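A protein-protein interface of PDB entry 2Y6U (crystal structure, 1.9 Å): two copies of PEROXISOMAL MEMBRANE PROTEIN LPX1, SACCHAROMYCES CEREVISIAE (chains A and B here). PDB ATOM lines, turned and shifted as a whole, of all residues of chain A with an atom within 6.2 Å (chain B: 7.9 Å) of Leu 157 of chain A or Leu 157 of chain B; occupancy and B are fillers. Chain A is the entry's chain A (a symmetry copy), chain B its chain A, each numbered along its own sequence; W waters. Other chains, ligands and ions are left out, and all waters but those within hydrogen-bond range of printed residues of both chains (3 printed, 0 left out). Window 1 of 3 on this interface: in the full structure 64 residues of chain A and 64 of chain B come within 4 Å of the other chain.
Arg 119 of chain A touches Leu 157 of chain B, and with the chains exchanged Leu 157 of chain A touches Arg 119 of chain B.
Arg 119 of chain A touches Gln 158 of chain B, and with the chains exchanged Gln 158 of chain A touches Arg 119 of chain B.
Arg 119 of chain A touches Pro 159 of chain B, and with the chains exchanged Pro 159 of chain A touches Arg 119 of chain B.
Val 156 of chain A touches Phe 275 of chain B, and with the chains exchanged Phe 275 of chain A touches Val 156 of chain B.
Positions printed for both chains: 115, 118, 119, 122, 152, 153, 154, 155, 156, 157, 158, 159 and 275.
Of the 12 pairs that touch across the chains among the printed residues, 9 have their exchanged pair printed and touching as well.
Hydrophobic or aromatic side chains of chain A that line the printed part of chain B: Val 156, Leu 157, Pro 159 and Phe 275.
Hydrophobic or aromatic side chains of chain B that line the printed part of chain A: Pro 18, Val 156, Leu 157, Pro 159 and Phe 275.
Among the printed residues, 12 pairs touch across the chains.
Among the printed residues, no Asp or Glu carboxylate lies within 4 Å of a Lys or Arg side-chain nitrogen of the other chain.
Gln 158 of chain B touches Arg 119 of chain A.
NH1 of Arg 119 of chain A touches CD of Pro 159 of chain B, at 3.8 Å.
Asn 160 of chain B touches Arg 119 of chain A (ND2 to NH2, 3.996 Å).
O of Val 156 of chain A touches CZ of Phe 275 of chain B, at 3.8 Å.
Leu 157 of chain A touches Leu 157 of chain B.
Gln 158 of chain A touches Arg 119 of chain B.
NH1 of Arg 119 of chain B touches CD of Pro 159 of chain A, 3.8 Å away.
Phe 275 of chain A touches Val 156 of chain B (CZ to O, 3.8 Å).
Phe 275 of chain A touches Asn 279 of chain B (CE1 to OD1, 3.9 Å).
The side-chain amide nitrogen (ND2) of Asn 279 of chain B sits at hydrogen-bond distance from the backbone carbonyl oxygen (O) of Phe 275 of chain B, at 2.8 Å.
The side-chain carboxylate (OD1) of Asp 116 of chain B is in salt-bridge range of the guanidinium group (NH2) of Arg 119 of chain B.
N of Asn 160 of chain B is in hydrogen-bond range of OE1 of Gln 158 of chain B, 2.9 Å away.
The backbone carbonyl oxygen (O) of Leu 157 of chain B sits at hydrogen-bond distance from the guanidinium group (NH1) of Arg 119 of chain A (2.9 Å).
O of Pro 18 of chain B is in hydrogen-bond range of NE2 of Gln 158 of chain A (2.9 Å).
The backbone carbonyl oxygen (O) of Leu 157 of chain A sits at hydrogen-bond distance from the guanidinium group (NH1) of Arg 119 of chain B.
Water W3 lies within hydrogen-bond range of the guanidinium group of Arg 119 of chain B (2.7 Å) and the backbone carbonyl oxygen of Val 156 of chain A (2.9 Å).
Water W1 lies within hydrogen-bond range of NH1 of Arg 119 of chain A and O of Val 156 of chain B.
Water W2 bridges ND2 of Asn 160 of chain B (2.8 Å) and NH2 of Arg 119 of chain A (3.2 Å).
Of the printed residues of chain B, Val 156 of chain A touches Phe 275.
Leu 157 of chain A touches just these residues of chain B: Arg 119 (2.9 Å) and Leu 157 (3.6 Å).
Ala 151 of chain B touches none of the printed residues of chain A.
Leu 157 of chain B touches just these residues of chain A: Arg 119 (2.9 Å) and Leu 157 (3.6 Å).
Printed residues of chain A within 4 Å of Asn 279 of chain B: Phe 275.
Val 283 of chain B touches none of the printed residues of chain A.
The nearest printed residue of chain A that does not touch Asn 279 of chain B is Val 156 of chain A (5.9 Å).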
ATOM      1  N   ILE A 115       9.437  16.205  -0.051  1.00  0.00           N
ATOM      2  CA  ILE A 115       8.001  15.927  -0.188  1.00  0.00           C
ATOM      3  C   ILE A 115       7.775  14.467  -0.656  1.00  0.00           C
ATOM      4  O   ILE A 115       6.865  13.781  -0.183  1.00  0.00           O
ATOM      5  CB  ILE A 115       7.265  16.912  -1.004  1.00  0.00           C
ATOM      6  CG1 ILE A 115       7.428  18.360  -0.456  1.00  0.00           C
ATOM      7  CG2 ILE A 115       5.710  16.529  -1.030  1.00  0.00           C
ATOM      8  CD1 ILE A 115       6.902  19.444  -1.344  1.00  0.00           C
ATOM      9  N   ALA A 118       8.049  12.570   2.392  1.00  0.00           N
ATOM     10  CA  ALA A 118       6.779  12.582   3.095  1.00  0.00           C
ATOM     11  C   ALA A 118       5.764  11.645   2.513  1.00  0.00           C
ATOM     12  O   ALA A 118       5.048  10.914   3.280  1.00  0.00           O
ATOM     13  CB  ALA A 118       6.194  14.032   3.247  1.00  0.00           C
ATOM     14  N   ARG A 119       5.684  11.560   1.198  1.00  0.00           N
ATOM     15  CA  ARG A 119       4.887  10.511   0.602  1.00  0.00           C
ATOM     16  C   ARG A 119       5.296   9.057   1.060  1.00  0.00           C
ATOM     17  O   ARG A 119       4.413   8.167   1.189  1.00  0.00           O
ATOM     18  CB  ARG A 119       4.792  10.616  -0.956  1.00  0.00           C
ATOM     19  CG  ARG A 119       4.005  11.830  -1.470  1.00  0.00           C
ATOM     20  CD  ARG A 119       3.578  11.922  -2.966  1.00  0.00           C
ATOM     21  NE  ARG A 119       4.709  12.617  -3.531  1.00  0.00           N
ATOM     22  CZ  ARG A 119       4.827  13.896  -3.755  1.00  0.00           C
ATOM     23  NH1 ARG A 119       3.918  14.731  -3.581  1.00  0.00           N
ATOM     24  NH2 ARG A 119       5.987  14.330  -4.076  1.00  0.00           N
ATOM     25  N   LEU A 122       3.898   8.538   4.498  1.00  0.00           N
ATOM     26  CA  LEU A 122       2.475   8.258   4.447  1.00  0.00           C
ATOM     27  C   LEU A 122       2.198   6.819   3.987  1.00  0.00           C
ATOM     28  O   LEU A 122       1.279   6.169   4.489  1.00  0.00           O
ATOM     29  CB  LEU A 122       1.743   9.237   3.556  1.00  0.00           C
ATOM     30  CG  LEU A 122       1.696  10.686   4.159  1.00  0.00           C
ATOM     31  CD1 LEU A 122       1.071  11.616   3.035  1.00  0.00           C
ATOM     32  CD2 LEU A 122       0.868  10.724   5.435  1.00  0.00           C
ATOM     33  N   LEU A 152       5.038  18.166   8.769  1.00  0.00           N
ATOM     34  CA  LEU A 152       4.132  19.147   8.185  1.00  0.00           C
ATOM     35  C   LEU A 152       3.593  18.750   6.806  1.00  0.00           C
ATOM     36  O   LEU A 152       2.385  18.798   6.554  1.00  0.00           O
ATOM     37  CB  LEU A 152       4.825  20.525   8.094  1.00  0.00           C
ATOM     38  CG  LEU A 152       5.124  21.226   9.385  1.00  0.00           C
ATOM     39  CD1 LEU A 152       6.171  22.400   9.204  1.00  0.00           C
ATOM     40  CD2 LEU A 152       3.779  21.750  10.010  1.00  0.00           C
ATOM     41  N   ALA A 153       4.491  18.266   5.941  1.00  0.00           N
ATOM     42  CA  ALA A 153       4.081  17.872   4.612  1.00  0.00           C
ATOM     43  C   ALA A 153       3.154  16.670   4.623  1.00  0.00           C
ATOM     44  O   ALA A 153       2.235  16.612   3.825  1.00  0.00           O
ATOM     45  CB  ALA A 153       5.318  17.600   3.691  1.00  0.00           C
ATOM     46  N   CYS A 154       3.382  15.749   5.562  1.00  0.00           N
ATOM     47  CA  CYS A 154       2.444  14.651   5.759  1.00  0.00           C
ATOM     48  C   CYS A 154       1.055  15.137   5.996  1.00  0.00           C
ATOM     49  O   CYS A 154       0.100  14.632   5.366  1.00  0.00           O
ATOM     50  CB  CYS A 154       2.830  13.769   6.965  1.00  0.00           C
ATOM     51  SG  CYS A 154       4.257  12.651   6.542  1.00  0.00           S
ATOM     52  N   ASP A 155       0.899  16.083   6.869  1.00  0.00           N
ATOM     53  CA  ASP A 155      -0.465  16.590   7.164  1.00  0.00           C
ATOM     54  C   ASP A 155      -1.061  17.297   5.985  1.00  0.00           C
ATOM     55  O   ASP A 155      -2.284  17.155   5.705  1.00  0.00           O
ATOM     56  CB  ASP A 155      -0.474  17.473   8.401  1.00  0.00           C
ATOM     57  CG  ASP A 155      -1.910  17.780   8.881  1.00  0.00           C
ATOM     58  OD1 ASP A 155      -2.513  16.815   9.415  1.00  0.00           O
ATOM     59  OD2 ASP A 155      -2.431  18.893   8.593  1.00  0.00           O
ATOM     60  N   VAL A 156      -0.234  18.040   5.205  1.00  0.00           N
ATOM     61  CA  VAL A 156      -0.707  18.705   4.043  1.00  0.00           C
ATOM     62  C   VAL A 156      -1.282  17.728   3.028  1.00  0.00           C
ATOM     63  O   VAL A 156      -2.355  17.945   2.432  1.00  0.00           O
ATOM     64  CB  VAL A 156       0.401  19.615   3.399  1.00  0.00           C
ATOM     65  CG1 VAL A 156      -0.088  20.108   2.007  1.00  0.00           C
ATOM     66  CG2 VAL A 156       0.742  20.862   4.389  1.00  0.00           C
ATOM     67  N   LEU A 157      -0.546  16.650   2.800  1.00  0.00           N
ATOM     68  CA  LEU A 157      -0.900  15.723   1.775  1.00  0.00           C
ATOM     69  C   LEU A 157      -2.005  14.720   2.234  1.00  0.00           C
ATOM     70  O   LEU A 157      -2.610  14.092   1.402  1.00  0.00           O
ATOM     71  CB  LEU A 157       0.327  14.868   1.390  1.00  0.00           C
ATOM     72  CG  LEU A 157       1.418  15.735   0.689  1.00  0.00           C
ATOM     73  CD1 LEU A 157       2.674  14.835   0.464  1.00  0.00           C
ATOM     74  CD2 LEU A 157       0.854  16.340  -0.646  1.00  0.00           C
ATOM     75  N   GLN A 158      -2.157  14.557   3.536  1.00  0.00           N
ATOM     76  CA  GLN A 158      -3.114  13.572   4.110  1.00  0.00           C
ATOM     77  C   GLN A 158      -3.501  14.110   5.533  1.00  0.00           C
ATOM     78  O   GLN A 158      -2.933  13.704   6.530  1.00  0.00           O
ATOM     79  CB  GLN A 158      -2.427  12.252   4.193  1.00  0.00           C
ATOM     80  CG  GLN A 158      -3.305  11.082   4.897  1.00  0.00           C
ATOM     81  CD  GLN A 158      -4.728  11.135   4.534  1.00  0.00           C
ATOM     82  OE1 GLN A 158      -5.486  11.948   5.087  1.00  0.00           O
ATOM     83  NE2 GLN A 158      -5.145  10.288   3.565  1.00  0.00           N
ATOM     84  N   PRO A 159      -4.442  15.008   5.609  1.00  0.00           N
ATOM     85  CA  PRO A 159      -4.697  15.647   6.831  1.00  0.00           C
ATOM     86  C   PRO A 159      -5.587  14.819   7.797  1.00  0.00           C
ATOM     87  O   PRO A 159      -5.996  15.311   8.872  1.00  0.00           O
ATOM     88  CB  PRO A 159      -5.447  16.940   6.364  1.00  0.00           C
ATOM     89  CG  PRO A 159      -6.213  16.533   5.236  1.00  0.00           C
ATOM     90  CD  PRO A 159      -5.221  15.632   4.536  1.00  0.00           C
ATOM     91  N   PHE A 275       6.280  24.942  -1.892  1.00  0.00           N
ATOM     92  CA  PHE A 275       5.011  24.187  -1.805  1.00  0.00           C
ATOM     93  C   PHE A 275       4.579  23.979  -0.348  1.00  0.00           C
ATOM     94  O   PHE A 275       3.458  24.252   0.039  1.00  0.00           O
ATOM     95  CB  PHE A 275       5.153  22.847  -2.498  1.00  0.00           C
ATOM     96  CG  PHE A 275       3.869  21.995  -2.373  1.00  0.00           C
ATOM     97  CD1 PHE A 275       2.817  22.208  -3.217  1.00  0.00           C
ATOM     98  CD2 PHE A 275       3.714  21.146  -1.343  1.00  0.00           C
ATOM     99  CE1 PHE A 275       1.635  21.438  -3.085  1.00  0.00           C
ATOM    100  CE2 PHE A 275       2.559  20.369  -1.230  1.00  0.00           C
ATOM    101  CZ  PHE A 275       1.544  20.525  -2.099  1.00  0.00           C
ATOM    102  N   PRO B  18      -6.329   7.284   5.514  1.00  0.00           N
ATOM    103  CA  PRO B  18      -7.604   7.715   6.063  1.00  0.00           C
ATOM    104  C   PRO B  18      -8.286   8.733   5.201  1.00  0.00           C
ATOM    105  O   PRO B  18      -7.753   9.111   4.167  1.00  0.00           O
ATOM    106  CB  PRO B  18      -7.236   8.288   7.445  1.00  0.00           C
ATOM    107  CG  PRO B  18      -5.847   8.776   7.262  1.00  0.00           C
ATOM    108  CD  PRO B  18      -5.203   7.861   6.224  1.00  0.00           C
ATOM    109  N   TRP B 114     -13.783  15.694  -2.151  1.00  0.00           N
ATOM    110  CA  TRP B 114     -13.330  15.340  -3.505  1.00  0.00           C
ATOM    111  C   TRP B 114     -11.818  15.115  -3.505  1.00  0.00           C
ATOM    112  O   TRP B 114     -11.323  14.422  -4.420  1.00  0.00           O
ATOM    113  CB  TRP B 114     -13.673  16.442  -4.499  1.00  0.00           C
ATOM    114  CG  TRP B 114     -15.110  16.657  -4.759  1.00  0.00           C
ATOM    115  CD1 TRP B 114     -16.176  15.982  -4.193  1.00  0.00           C
ATOM    116  CD2 TRP B 114     -15.646  17.542  -5.688  1.00  0.00           C
ATOM    117  NE1 TRP B 114     -17.356  16.504  -4.650  1.00  0.00           N
ATOM    118  CE2 TRP B 114     -17.077  17.393  -5.639  1.00  0.00           C
ATOM    119  CE3 TRP B 114     -15.099  18.486  -6.563  1.00  0.00           C
ATOM    120  CZ2 TRP B 114     -17.917  18.157  -6.412  1.00  0.00           C
ATOM    121  CZ3 TRP B 114     -15.906  19.165  -7.392  1.00  0.00           C
ATOM    122  CH2 TRP B 114     -17.355  19.068  -7.269  1.00  0.00           C
ATOM    123  N   ILE B 115     -11.097  15.695  -2.526  1.00  0.00           N
ATOM    124  CA  ILE B 115      -9.648  15.490  -2.396  1.00  0.00           C
ATOM    125  C   ILE B 115      -9.344  14.030  -1.974  1.00  0.00           C
ATOM    126  O   ILE B 115      -8.399  13.409  -2.469  1.00  0.00           O
ATOM    127  CB  ILE B 115      -8.965  16.487  -1.549  1.00  0.00           C
ATOM    128  CG1 ILE B 115      -9.205  17.941  -2.052  1.00  0.00           C
ATOM    129  CG2 ILE B 115      -7.392  16.186  -1.534  1.00  0.00           C
ATOM    130  CD1 ILE B 115      -8.738  19.022  -1.129  1.00  0.00           C
ATOM    131  N   ASP B 116     -10.131  13.493  -1.064  1.00  0.00           N
ATOM    132  CA  ASP B 116     -10.087  12.024  -0.739  1.00  0.00           C
ATOM    133  C   ASP B 116     -10.281  11.224  -2.046  1.00  0.00           C
ATOM    134  O   ASP B 116      -9.564  10.246  -2.301  1.00  0.00           O
ATOM    135  CB  ASP B 116     -11.171  11.615   0.226  1.00  0.00           C
ATOM    136  CG  ASP B 116     -11.004  12.185   1.620  1.00  0.00           C
ATOM    137  OD1 ASP B 116     -10.040  12.923   1.942  1.00  0.00           O
ATOM    138  OD2 ASP B 116     -11.971  11.950   2.455  1.00  0.00           O
ATOM    139  N   GLY B 117     -11.248  11.611  -2.859  1.00  0.00           N
ATOM    140  CA  GLY B 117     -11.468  10.961  -4.132  1.00  0.00           C
ATOM    141  C   GLY B 117     -10.221  11.068  -5.082  1.00  0.00           C
ATOM    142  O   GLY B 117      -9.908  10.138  -5.792  1.00  0.00           O
ATOM    143  N   ALA B 118      -9.519  12.219  -5.081  1.00  0.00           N
ATOM    144  CA  ALA B 118      -8.252  12.321  -5.782  1.00  0.00           C
ATOM    145  C   ALA B 118      -7.188  11.421  -5.230  1.00  0.00           C
ATOM    146  O   ALA B 118      -6.434  10.754  -6.019  1.00  0.00           O
ATOM    147  CB  ALA B 118      -7.745  13.803  -5.889  1.00  0.00           C
ATOM    148  N   ARG B 119      -7.103  11.299  -3.917  1.00  0.00           N
ATOM    149  CA  ARG B 119      -6.250  10.276  -3.354  1.00  0.00           C
ATOM    150  C   ARG B 119      -6.581   8.817  -3.859  1.00  0.00           C
ATOM    151  O   ARG B 119      -5.652   7.980  -4.015  1.00  0.00           O
ATOM    152  CB  ARG B 119      -6.159  10.337  -1.794  1.00  0.00           C
ATOM    153  CG  ARG B 119      -5.438  11.574  -1.241  1.00  0.00           C
ATOM    154  CD  ARG B 119      -5.015  11.641   0.258  1.00  0.00           C
ATOM    155  NE  ARG B 119      -6.181  12.256   0.844  1.00  0.00           N
ATOM    156  CZ  ARG B 119      -6.367  13.520   1.108  1.00  0.00           C
ATOM    157  NH1 ARG B 119      -5.504  14.407   0.961  1.00  0.00           N
ATOM    158  NH2 ARG B 119      -7.548  13.881   1.441  1.00  0.00           N
ATOM    159  N   ASP B 120      -7.845   8.529  -4.038  1.00  0.00           N
ATOM    160  CA  ASP B 120      -8.267   7.219  -4.575  1.00  0.00           C
ATOM    161  C   ASP B 120      -7.741   7.004  -6.010  1.00  0.00           C
ATOM    162  O   ASP B 120      -7.215   5.938  -6.353  1.00  0.00           O
ATOM    163  CB  ASP B 120      -9.792   7.160  -4.581  1.00  0.00           C
ATOM    164  CG  ASP B 120     -10.373   7.126  -3.140  1.00  0.00           C
ATOM    165  OD1 ASP B 120      -9.639   6.741  -2.199  1.00  0.00           O
ATOM    166  OD2 ASP B 120     -11.546   7.541  -2.994  1.00  0.00           O
ATOM    167  N   LEU B 122      -5.160   8.482  -7.310  1.00  0.00           N
ATOM    168  CA  LEU B 122      -3.724   8.277  -7.267  1.00  0.00           C
ATOM    169  C   LEU B 122      -3.370   6.841  -6.852  1.00  0.00           C
ATOM    170  O   LEU B 122      -2.419   6.258  -7.374  1.00  0.00           O
ATOM    171  CB  LEU B 122      -3.045   9.265  -6.345  1.00  0.00           C
ATOM    172  CG  LEU B 122      -3.076  10.733  -6.901  1.00  0.00           C
ATOM    173  CD1 LEU B 122      -2.501  11.659  -5.748  1.00  0.00           C
ATOM    174  CD2 LEU B 122      -2.252  10.856  -8.175  1.00  0.00           C
ATOM    175  N   GLN B 150     -10.685  16.959  -9.549  1.00  0.00           N
ATOM    176  CA  GLN B 150      -9.826  15.861  -9.085  1.00  0.00           C
ATOM    177  C   GLN B 150      -8.568  15.660  -9.885  1.00  0.00           C
ATOM    178  O   GLN B 150      -7.553  15.385  -9.307  1.00  0.00           O
ATOM    179  CB  GLN B 150     -10.623  14.578  -8.940  1.00  0.00           C
ATOM    180  CG  GLN B 150     -11.689  14.711  -7.854  1.00  0.00           C
ATOM    181  CD  GLN B 150     -12.567  13.491  -7.769  1.00  0.00           C
ATOM    182  OE1 GLN B 150     -13.000  12.963  -8.795  1.00  0.00           O
ATOM    183  NE2 GLN B 150     -12.886  13.074  -6.565  1.00  0.00           N
ATOM    184  N   ALA B 151      -8.631  15.951 -11.180  1.00  0.00           N
ATOM    185  CA  ALA B 151      -7.427  15.941 -12.032  1.00  0.00           C
ATOM    186  C   ALA B 151      -6.385  16.923 -11.506  1.00  0.00           C
ATOM    187  O   ALA B 151      -5.226  16.608 -11.413  1.00  0.00           O
ATOM    188  CB  ALA B 151      -7.779  16.244 -13.507  1.00  0.00           C
ATOM    189  N   LEU B 152      -6.817  18.166 -11.276  1.00  0.00           N
ATOM    190  CA  LEU B 152      -5.963  19.175 -10.661  1.00  0.00           C
ATOM    191  C   LEU B 152      -5.404  18.764  -9.294  1.00  0.00           C
ATOM    192  O   LEU B 152      -4.200  18.868  -9.039  1.00  0.00           O
ATOM    193  CB  LEU B 152      -6.729  20.510 -10.526  1.00  0.00           C
ATOM    194  CG  LEU B 152      -7.067  21.235 -11.795  1.00  0.00           C
ATOM    195  CD1 LEU B 152      -8.175  22.345 -11.578  1.00  0.00           C
ATOM    196  CD2 LEU B 152      -5.752  21.850 -12.402  1.00  0.00           C
ATOM    197  N   ALA B 153      -6.273  18.205  -8.446  1.00  0.00           N
ATOM    198  CA  ALA B 153      -5.842  17.792  -7.129  1.00  0.00           C
ATOM    199  C   ALA B 153      -4.852  16.643  -7.178  1.00  0.00           C
ATOM    200  O   ALA B 153      -3.930  16.609  -6.381  1.00  0.00           O
ATOM    201  CB  ALA B 153      -7.061  17.426  -6.218  1.00  0.00           C
ATOM    202  N   CYS B 154      -5.031  15.741  -8.146  1.00  0.00           N
ATOM    203  CA  CYS B 154      -4.036  14.701  -8.376  1.00  0.00           C
ATOM    204  C   CYS B 154      -2.675  15.267  -8.596  1.00  0.00           C
ATOM    205  O   CYS B 154      -1.694  14.795  -7.982  1.00  0.00           O
ATOM    206  CB  CYS B 154      -4.375  13.838  -9.610  1.00  0.00           C
ATOM    207  SG  CYS B 154      -5.740  12.633  -9.224  1.00  0.00           S
ATOM    208  N   ASP B 155      -2.571  16.248  -9.439  1.00  0.00           N
ATOM    209  CA  ASP B 155      -1.236  16.836  -9.717  1.00  0.00           C
ATOM    210  C   ASP B 155      -0.677  17.537  -8.516  1.00  0.00           C
ATOM    211  O   ASP B 155       0.551  17.451  -8.239  1.00  0.00           O
ATOM    212  CB  ASP B 155      -1.275  17.757 -10.925  1.00  0.00           C
ATOM    213  CG  ASP B 155       0.142  18.155 -11.394  1.00  0.00           C
ATOM    214  OD1 ASP B 155       0.795  17.241 -11.957  1.00  0.00           O
ATOM    215  OD2 ASP B 155       0.603  19.285 -11.071  1.00  0.00           O
ATOM    216  N   VAL B 156      -1.542  18.209  -7.713  1.00  0.00           N
ATOM    217  CA  VAL B 156      -1.105  18.862  -6.530  1.00  0.00           C
ATOM    218  C   VAL B 156      -0.477  17.885  -5.546  1.00  0.00           C
ATOM    219  O   VAL B 156       0.583  18.140  -4.943  1.00  0.00           O
ATOM    220  CB  VAL B 156      -2.259  19.691  -5.859  1.00  0.00           C
ATOM    221  CG1 VAL B 156      -1.796  20.165  -4.451  1.00  0.00           C
ATOM    222  CG2 VAL B 156      -2.667  20.948  -6.810  1.00  0.00           C
ATOM    223  N   LEU B 157      -1.155  16.763  -5.353  1.00  0.00           N
ATOM    224  CA  LEU B 157      -0.751  15.824  -4.357  1.00  0.00           C
ATOM    225  C   LEU B 157       0.407  14.896  -4.847  1.00  0.00           C
ATOM    226  O   LEU B 157       1.045  14.275  -4.035  1.00  0.00           O
ATOM    227  CB  LEU B 157      -1.930  14.893  -4.001  1.00  0.00           C
ATOM    228  CG  LEU B 157      -3.065  15.678  -3.274  1.00  0.00           C
ATOM    229  CD1 LEU B 157      -4.271  14.705  -3.078  1.00  0.00           C
ATOM    230  CD2 LEU B 157      -2.533  16.269  -1.920  1.00  0.00           C
ATOM    231  N   GLN B 158       0.566  14.783  -6.153  1.00  0.00           N
ATOM    232  CA  GLN B 158       1.573  13.869  -6.757  1.00  0.00           C
ATOM    233  C   GLN B 158       1.929  14.471  -8.162  1.00  0.00           C
ATOM    234  O   GLN B 158       1.383  14.067  -9.172  1.00  0.00           O
ATOM    235  CB  GLN B 158       0.957  12.517  -6.882  1.00  0.00           C
ATOM    236  CG  GLN B 158       1.896  11.419  -7.622  1.00  0.00           C
ATOM    237  CD  GLN B 158       3.315  11.537  -7.257  1.00  0.00           C
ATOM    238  OE1 GLN B 158       4.027  12.405  -7.783  1.00  0.00           O
ATOM    239  NE2 GLN B 158       3.777  10.683  -6.314  1.00  0.00           N
ATOM    240  N   PRO B 159       2.821  15.420  -8.209  1.00  0.00           N
ATOM    241  CA  PRO B 159       3.041  16.111  -9.410  1.00  0.00           C
ATOM    242  C   PRO B 159       3.973  15.363 -10.401  1.00  0.00           C
ATOM    243  O   PRO B 159       4.354  15.909 -11.459  1.00  0.00           O
ATOM    244  CB  PRO B 159       3.721  17.426  -8.902  1.00  0.00           C
ATOM    245  CG  PRO B 159       4.509  17.026  -7.787  1.00  0.00           C
ATOM    246  CD  PRO B 159       3.566  16.051  -7.116  1.00  0.00           C
ATOM    247  N   ASN B 160       4.281  14.102 -10.151  1.00  0.00           N
ATOM    248  CA  ASN B 160       5.206  13.406 -11.032  1.00  0.00           C
ATOM    249  C   ASN B 160       4.497  12.353 -11.868  1.00  0.00           C
ATOM    250  O   ASN B 160       5.127  11.564 -12.525  1.00  0.00           O
ATOM    251  CB  ASN B 160       6.266  12.799 -10.150  1.00  0.00           C
ATOM    252  CG  ASN B 160       6.940  13.798  -9.313  1.00  0.00           C
ATOM    253  OD1 ASN B 160       7.605  14.685  -9.854  1.00  0.00           O
ATOM    254  ND2 ASN B 160       6.819  13.683  -7.931  1.00  0.00           N
ATOM    255  N   PHE B 275      -8.410  24.525  -0.407  1.00  0.00           N
ATOM    256  CA  PHE B 275      -7.102  23.843  -0.517  1.00  0.00           C
ATOM    257  C   PHE B 275      -6.661  23.704  -1.979  1.00  0.00           C
ATOM    258  O   PHE B 275      -5.556  24.049  -2.356  1.00  0.00           O
ATOM    259  CB  PHE B 275      -7.171  22.476   0.134  1.00  0.00           C
ATOM    260  CG  PHE B 275      -5.844  21.698  -0.018  1.00  0.00           C
ATOM    261  CD1 PHE B 275      -4.805  21.940   0.834  1.00  0.00           C
ATOM    262  CD2 PHE B 275      -5.645  20.892  -1.074  1.00  0.00           C
ATOM    263  CE1 PHE B 275      -3.583  21.239   0.678  1.00  0.00           C
ATOM    264  CE2 PHE B 275      -4.450  20.182  -1.210  1.00  0.00           C
ATOM    265  CZ  PHE B 275      -3.444  20.364  -0.336  1.00  0.00           C
ATOM    266  N   LEU B 276      -7.588  23.313  -2.850  1.00  0.00           N
ATOM    267  CA  LEU B 276      -7.335  23.183  -4.282  1.00  0.00           C
ATOM    268  C   LEU B 276      -7.067  24.537  -4.917  1.00  0.00           C
ATOM    269  O   LEU B 276      -6.028  24.724  -5.576  1.00  0.00           O
ATOM    270  CB  LEU B 276      -8.418  22.372  -5.016  1.00  0.00           C
ATOM    271  CG  LEU B 276      -7.910  22.362  -6.487  1.00  0.00           C
ATOM    272  CD1 LEU B 276      -6.629  21.404  -6.614  1.00  0.00           C
ATOM    273  CD2 LEU B 276      -8.829  22.348  -7.568  1.00  0.00           C
ATOM    274  N   ASN B 279      -3.667  26.010  -4.420  1.00  0.00           N
ATOM    275  CA  ASN B 279      -2.634  25.192  -4.999  1.00  0.00           C
ATOM    276  C   ASN B 279      -2.602  25.060  -6.494  1.00  0.00           C
ATOM    277  O   ASN B 279      -1.654  24.453  -7.081  1.00  0.00           O
ATOM    278  CB  ASN B 279      -2.591  23.808  -4.312  1.00  0.00           C
ATOM    279  CG  ASN B 279      -2.004  23.937  -2.970  1.00  0.00           C
ATOM    280  OD1 ASN B 279      -0.859  24.428  -2.859  1.00  0.00           O
ATOM    281  ND2 ASN B 279      -2.777  23.685  -1.898  1.00  0.00           N
ATOM    282  N   VAL B 283       0.403  23.771 -10.271  1.00  0.00           N
ATOM    283  CA  VAL B 283       0.126  22.837 -11.357  1.00  0.00           C
ATOM    284  C   VAL B 283       0.818  23.410 -12.619  1.00  0.00           C
ATOM    285  O   VAL B 283       0.339  24.368 -13.221  1.00  0.00           O
ATOM    286  CB  VAL B 283      -1.378  22.639 -11.601  1.00  0.00           C
ATOM    287  CG1 VAL B 283      -1.650  21.797 -12.895  1.00  0.00           C
ATOM    288  CG2 VAL B 283      -2.002  21.974 -10.301  1.00  0.00           C
HETATM  289  O   HOH W   1       3.007  17.290  -3.668  1.00  0.00           O
HETATM  290  O   HOH W   2       7.939  15.587  -6.233  1.00  0.00           O
HETATM  291  O   HOH W   3      -4.731  17.008   1.129  1.00  0.00           O
